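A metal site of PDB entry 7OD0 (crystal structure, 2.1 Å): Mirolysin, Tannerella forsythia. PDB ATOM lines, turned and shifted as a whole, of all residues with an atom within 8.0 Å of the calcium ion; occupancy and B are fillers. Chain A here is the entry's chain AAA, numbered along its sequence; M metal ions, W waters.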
ATOM      1  N   HIS A 180       1.422 -17.965  23.057  1.00  0.00           N
ATOM      2  CA  HIS A 180       2.816 -17.664  23.454  1.00  0.00           C
ATOM      3  C   HIS A 180       2.812 -16.669  24.620  1.00  0.00           C
ATOM      4  O   HIS A 180       2.123 -15.615  24.532  1.00  0.00           O
ATOM      5  CB  HIS A 180       3.638 -17.135  22.264  1.00  0.00           C
ATOM      6  CG  HIS A 180       3.854 -18.175  21.221  1.00  0.00           C
ATOM      7  ND1 HIS A 180       3.894 -17.884  19.891  1.00  0.00           N
ATOM      8  CD2 HIS A 180       4.074 -19.509  21.335  1.00  0.00           C
ATOM      9  CE1 HIS A 180       4.130 -18.976  19.205  1.00  0.00           C
ATOM     10  NE2 HIS A 180       4.250 -19.996  20.060  1.00  0.00           N
ATOM     11  N   ILE A 181       3.581 -17.005  25.660  1.00  0.00           N
ATOM     12  CA  ILE A 181       3.592 -16.281  26.951  1.00  0.00           C
ATOM     13  C   ILE A 181       4.021 -14.832  26.729  1.00  0.00           C
ATOM     14  O   ILE A 181       3.604 -13.988  27.546  1.00  0.00           O
ATOM     15  CB  ILE A 181       4.495 -17.007  27.973  1.00  0.00           C
ATOM     16  CG1 ILE A 181       4.355 -16.409  29.373  1.00  0.00           C
ATOM     17  CG2 ILE A 181       5.938 -17.026  27.500  1.00  0.00           C
ATOM     18  CD1 ILE A 181       4.953 -17.263  30.440  1.00  0.00           C
ATOM     19  N   TRP A 182       4.818 -14.539  25.688  1.00  0.00           N
ATOM     20  CA  TRP A 182       5.354 -13.174  25.423  1.00  0.00           C
ATOM     21  C   TRP A 182       4.343 -12.358  24.575  1.00  0.00           C
ATOM     22  O   TRP A 182       4.547 -11.145  24.408  1.00  0.00           O
ATOM     23  CB  TRP A 182       6.755 -13.266  24.775  1.00  0.00           C
ATOM     24  CG  TRP A 182       6.757 -13.771  23.375  1.00  0.00           C
ATOM     25  CD1 TRP A 182       6.677 -13.004  22.257  1.00  0.00           C
ATOM     26  CD2 TRP A 182       6.857 -15.124  22.919  1.00  0.00           C
ATOM     27  NE1 TRP A 182       6.683 -13.789  21.129  1.00  0.00           N
ATOM     28  CE2 TRP A 182       6.799 -15.097  21.511  1.00  0.00           C
ATOM     29  CE3 TRP A 182       6.995 -16.371  23.545  1.00  0.00           C
ATOM     30  CZ2 TRP A 182       6.852 -16.266  20.737  1.00  0.00           C
ATOM     31  CZ3 TRP A 182       7.036 -17.519  22.777  1.00  0.00           C
ATOM     32  CH2 TRP A 182       6.992 -17.458  21.391  1.00  0.00           C
ATOM     33  N   GLY A 183       3.278 -12.981  24.062  1.00  0.00           N
ATOM     34  CA  GLY A 183       2.187 -12.254  23.396  1.00  0.00           C
ATOM     35  C   GLY A 183       2.387 -12.061  21.902  1.00  0.00           C
ATOM     36  O   GLY A 183       1.658 -11.229  21.309  1.00  0.00           O
ATOM     37  N   ASP A 184       3.321 -12.774  21.273  1.00  0.00           N
ATOM     38  CA  ASP A 184       3.440 -12.736  19.789  1.00  0.00           C
ATOM     39  C   ASP A 184       3.524 -11.276  19.331  1.00  0.00           C
ATOM     40  O   ASP A 184       2.824 -10.896  18.385  1.00  0.00           O
ATOM     41  CB  ASP A 184       2.247 -13.483  19.137  1.00  0.00           C
ATOM     42  CG  ASP A 184       2.294 -14.968  19.404  1.00  0.00           C
ATOM     43  OD1 ASP A 184       3.378 -15.544  19.167  1.00  0.00           O
ATOM     44  OD2 ASP A 184       1.286 -15.533  19.862  1.00  0.00           O
ATOM     45  N   ASP A 185       4.382 -10.481  19.958  1.00  0.00           N
ATOM     46  CA  ASP A 185       4.462  -9.033  19.688  1.00  0.00           C
ATOM     47  C   ASP A 185       5.895  -8.649  19.340  1.00  0.00           C
ATOM     48  O   ASP A 185       6.219  -7.431  19.418  1.00  0.00           O
ATOM     49  CB  ASP A 185       3.926  -8.247  20.879  1.00  0.00           C
ATOM     50  CG  ASP A 185       4.596  -8.579  22.189  1.00  0.00           C
ATOM     51  OD1 ASP A 185       5.723  -9.154  22.148  1.00  0.00           O
ATOM     52  OD2 ASP A 185       4.000  -8.266  23.253  1.00  0.00           O
ATOM     53  N   GLY A 186       6.728  -9.647  18.976  1.00  0.00           N
ATOM     54  CA  GLY A 186       8.083  -9.449  18.447  1.00  0.00           C
ATOM     55  C   GLY A 186       8.990  -8.779  19.457  1.00  0.00           C
ATOM     56  O   GLY A 186       9.976  -8.207  19.020  1.00  0.00           O
ATOM     57  N   GLY A 187       8.667  -8.795  20.750  1.00  0.00           N
ATOM     58  CA  GLY A 187       9.552  -8.283  21.808  1.00  0.00           C
ATOM     59  C   GLY A 187       8.970  -7.141  22.642  1.00  0.00           C
ATOM     60  O   GLY A 187       9.603  -6.816  23.670  1.00  0.00           O
ATOM     61  N   SER A 188       7.820  -6.532  22.266  1.00  0.00           N
ATOM     62  CA  SER A 188       7.280  -5.354  22.986  1.00  0.00           C
ATOM     63  C   SER A 188       6.678  -5.809  24.311  1.00  0.00           C
ATOM     64  O   SER A 188       6.697  -7.037  24.563  1.00  0.00           O
ATOM     65  CB  SER A 188       6.230  -4.619  22.179  1.00  0.00           C
ATOM     66  OG  SER A 188       5.042  -5.382  22.104  1.00  0.00           O
ATOM     67  N   CYS A 189       6.168  -4.863  25.098  1.00  0.00           N
ATOM     68  CA  CYS A 189       5.367  -5.154  26.327  1.00  0.00           C
ATOM     69  C   CYS A 189       3.859  -5.064  26.033  1.00  0.00           C
ATOM     70  O   CYS A 189       3.069  -5.273  26.977  1.00  0.00           O
ATOM     71  CB  CYS A 189       5.765  -4.186  27.418  1.00  0.00           C
ATOM     72  SG  CYS A 189       7.546  -4.210  27.737  1.00  0.00           S
ATOM     73  N   SER A 190       3.458  -4.782  24.799  1.00  0.00           N
ATOM     74  CA  SER A 190       2.063  -4.417  24.404  1.00  0.00           C
ATOM     75  C   SER A 190       1.194  -5.676  24.267  1.00  0.00           C
ATOM     76  O   SER A 190       0.064  -5.640  24.765  1.00  0.00           O
ATOM     77  CB  SER A 190       2.017  -3.606  23.144  1.00  0.00           C
ATOM     78  OG  SER A 190       2.452  -2.285  23.371  1.00  0.00           O
ATOM     79  N   GLY A 191       1.660  -6.704  23.555  1.00  0.00           N
ATOM     80  CA  GLY A 191       0.927  -7.982  23.375  1.00  0.00           C
ATOM     81  C   GLY A 191       0.664  -8.682  24.704  1.00  0.00           C
ATOM     82  O   GLY A 191       1.377  -8.419  25.695  1.00  0.00           O
ATOM     83  N   THR A 192      -0.317  -9.574  24.731  1.00  0.00           N
ATOM     84  CA  THR A 192      -0.725 -10.341  25.926  1.00  0.00           C
ATOM     85  C   THR A 192      -1.052 -11.779  25.522  1.00  0.00           C
ATOM     86  O   THR A 192      -1.520 -11.966  24.420  1.00  0.00           O
ATOM     87  CB  THR A 192      -1.922  -9.673  26.619  1.00  0.00           C
ATOM     88  OG1 THR A 192      -2.252 -10.493  27.742  1.00  0.00           O
ATOM     89  CG2 THR A 192      -3.153  -9.542  25.756  1.00  0.00           C
ATOM     90  N   ASP A 193      -0.826 -12.739  26.413  1.00  0.00           N
ATOM     91  CA  ASP A 193      -1.303 -14.135  26.273  1.00  0.00           C
ATOM     92  C   ASP A 193      -2.681 -14.271  26.946  1.00  0.00           C
ATOM     93  O   ASP A 193      -3.232 -15.386  26.953  1.00  0.00           O
ATOM     94  CB  ASP A 193      -0.265 -15.116  26.830  1.00  0.00           C
ATOM     95  CG  ASP A 193      -0.047 -15.016  28.327  1.00  0.00           C
ATOM     96  OD1 ASP A 193      -0.524 -14.023  28.922  1.00  0.00           O
ATOM     97  OD2 ASP A 193       0.576 -15.937  28.881  1.00  0.00           O
ATOM     98  N   PRO A 199       3.760 -13.483  33.992  1.00  0.00           N
ATOM     99  CA  PRO A 199       4.319 -12.136  34.004  1.00  0.00           C
ATOM    100  C   PRO A 199       4.450 -11.585  32.580  1.00  0.00           C
ATOM    101  O   PRO A 199       4.743 -12.366  31.675  1.00  0.00           O
ATOM    102  CB  PRO A 199       5.724 -12.302  34.608  1.00  0.00           C
ATOM    103  CG  PRO A 199       5.675 -13.617  35.347  1.00  0.00           C
ATOM    104  CD  PRO A 199       4.658 -14.461  34.625  1.00  0.00           C
ATOM    105  N   ASN A 200       4.221 -10.282  32.412  1.00  0.00           N
ATOM    106  CA  ASN A 200       4.363  -9.618  31.098  1.00  0.00           C
ATOM    107  C   ASN A 200       5.798  -9.871  30.631  1.00  0.00           C
ATOM    108  O   ASN A 200       6.729  -9.864  31.486  1.00  0.00           O
ATOM    109  CB  ASN A 200       4.000  -8.130  31.152  1.00  0.00           C
ATOM    110  CG  ASN A 200       3.832  -7.522  29.777  1.00  0.00           C
ATOM    111  OD1 ASN A 200       3.569  -8.252  28.823  1.00  0.00           O
ATOM    112  ND2 ASN A 200       3.929  -6.212  29.653  1.00  0.00           N
ATOM    113  N   GLN A 201       6.004 -10.095  29.343  1.00  0.00           N
ATOM    114  CA  GLN A 201       7.315 -10.563  28.830  1.00  0.00           C
ATOM    115  C   GLN A 201       7.534  -9.966  27.443  1.00  0.00           C
ATOM    116  O   GLN A 201       6.565  -9.990  26.645  1.00  0.00           O
ATOM    117  CB  GLN A 201       7.329 -12.097  28.869  1.00  0.00           C
ATOM    118  CG  GLN A 201       8.466 -12.746  28.114  1.00  0.00           C
ATOM    119  CD  GLN A 201       8.508 -14.251  28.256  1.00  0.00           C
ATOM    120  OE1 GLN A 201       8.017 -14.847  29.228  1.00  0.00           O
ATOM    121  NE2 GLN A 201       9.099 -14.873  27.267  1.00  0.00           N
ATOM    122  N   GLY A 202       8.744  -9.491  27.146  1.00  0.00           N
ATOM    123  CA  GLY A 202       9.072  -8.858  25.856  1.00  0.00           C
ATOM    124  C   GLY A 202       9.001  -9.855  24.726  1.00  0.00           C
ATOM    125  O   GLY A 202       7.967  -9.907  24.039  1.00  0.00           O
ATOM    126  N   GLY A 203      10.047 -10.663  24.582  1.00  0.00           N
ATOM    127  CA  GLY A 203      10.157 -11.606  23.464  1.00  0.00           C
ATOM    128  C   GLY A 203      10.197 -13.021  23.981  1.00  0.00           C
ATOM    129  O   GLY A 203      10.119 -13.199  25.209  1.00  0.00           O
ATOM    130  N   TYR A 204      10.338 -13.985  23.086  1.00  0.00           N
ATOM    131  CA  TYR A 204      10.470 -15.419  23.434  1.00  0.00           C
ATOM    132  C   TYR A 204      11.850 -15.648  24.031  1.00  0.00           C
ATOM    133  O   TYR A 204      12.792 -14.894  23.743  1.00  0.00           O
ATOM    134  CB  TYR A 204      10.223 -16.331  22.230  1.00  0.00           C
ATOM    135  CG  TYR A 204      11.124 -16.150  21.035  1.00  0.00           C
ATOM    136  CD1 TYR A 204      12.402 -16.692  21.009  1.00  0.00           C
ATOM    137  CD2 TYR A 204      10.677 -15.526  19.885  1.00  0.00           C
ATOM    138  CE1 TYR A 204      13.218 -16.571  19.887  1.00  0.00           C
ATOM    139  CE2 TYR A 204      11.463 -15.404  18.756  1.00  0.00           C
ATOM    140  CZ  TYR A 204      12.749 -15.927  18.760  1.00  0.00           C
ATOM    141  OH  TYR A 204      13.530 -15.820  17.638  1.00  0.00           O
ATOM    142  N   ASP A 215      13.454  -8.588  31.678  1.00  0.00           N
ATOM    143  CA  ASP A 215      13.461  -7.785  30.428  1.00  0.00           C
ATOM    144  C   ASP A 215      12.818  -6.431  30.734  1.00  0.00           C
ATOM    145  O   ASP A 215      12.464  -6.184  31.915  1.00  0.00           O
ATOM    146  CB  ASP A 215      12.801  -8.547  29.263  1.00  0.00           C
ATOM    147  CG  ASP A 215      11.326  -8.883  29.432  1.00  0.00           C
ATOM    148  OD1 ASP A 215      10.629  -8.167  30.190  1.00  0.00           O
ATOM    149  OD2 ASP A 215      10.866  -9.872  28.789  1.00  0.00           O
ATOM    150  N   HIS A 216      12.650  -5.591  29.718  1.00  0.00           N
ATOM    151  CA  HIS A 216      12.101  -4.216  29.907  1.00  0.00           C
ATOM    152  C   HIS A 216      10.653  -4.276  30.396  1.00  0.00           C
ATOM    153  O   HIS A 216      10.227  -3.267  30.966  1.00  0.00           O
ATOM    154  CB  HIS A 216      12.328  -3.338  28.674  1.00  0.00           C
ATOM    155  CG  HIS A 216      11.582  -3.712  27.439  1.00  0.00           C
ATOM    156  ND1 HIS A 216      10.645  -2.857  26.844  1.00  0.00           N
ATOM    157  CD2 HIS A 216      11.680  -4.795  26.628  1.00  0.00           C
ATOM    158  CE1 HIS A 216      10.180  -3.420  25.746  1.00  0.00           C
ATOM    159  NE2 HIS A 216      10.801  -4.599  25.591  1.00  0.00           N
ATOM    160  N   CYS A 217       9.945  -5.407  30.229  1.00  0.00           N
ATOM    161  CA  CYS A 217       8.515  -5.582  30.639  1.00  0.00           C
ATOM    162  C   CYS A 217       8.399  -6.023  32.102  1.00  0.00           C
ATOM    163  O   CYS A 217       7.523  -5.484  32.782  1.00  0.00           O
ATOM    164  CB  CYS A 217       7.791  -6.589  29.764  1.00  0.00           C
ATOM    165  SG  CYS A 217       7.981  -6.243  27.998  1.00  0.00           S
HETATM  166 CA    CA M   1       5.718  -9.141  24.581  1.00  0.00          CA
HETATM  167  O   HOH W   1       4.193  -8.508  26.325  1.00  0.00           O
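Within 4 Å of the calcium ion: Trp 182, Asp 185, Ser 188, Gln 201 and Gly 202.
The calcium ion is bound by the backbone carbonyl oxygen (O) of Ser 188, the backbone carbonyl oxygen (O) of Trp 182, the side-chain carboxylate (OD2) of Asp 185, the backbone carbonyl oxygen (O) of Gln 201, water W1, the side-chain carboxylate (OD1) of Asp 185 and the backbone carbonyl oxygen (O) of Gly 202. The calcium ion has seven donor atoms within binding distance.
N of Ser 190 is in hydrogen-bond range of OG of Ser 188 (3.2 Å). The side-chain carboxylate (OD1) of Asp 185 sits close to the backbone NH (N) of Gly 187 (3.3 Å). The backbone NH (N) of Gly 191 lies close to the side-chain carboxylate (OD2) of Asp 185. The side-chain amide nitrogen (NE2) of Gln 201 lies within hydrogen-bond range of the backbone carbonyl oxygen (O) of Gly 203 (2.8 Å). N of Gly 202 is in hydrogen-bond range of SG of Cys 217 (3.4 Å). OD2 of Asp 215 is in hydrogen-bond range of N of Gly 202. SG of Cys 189 is disulfide-bonded to SG of Cys 217, at 2.1 Å.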
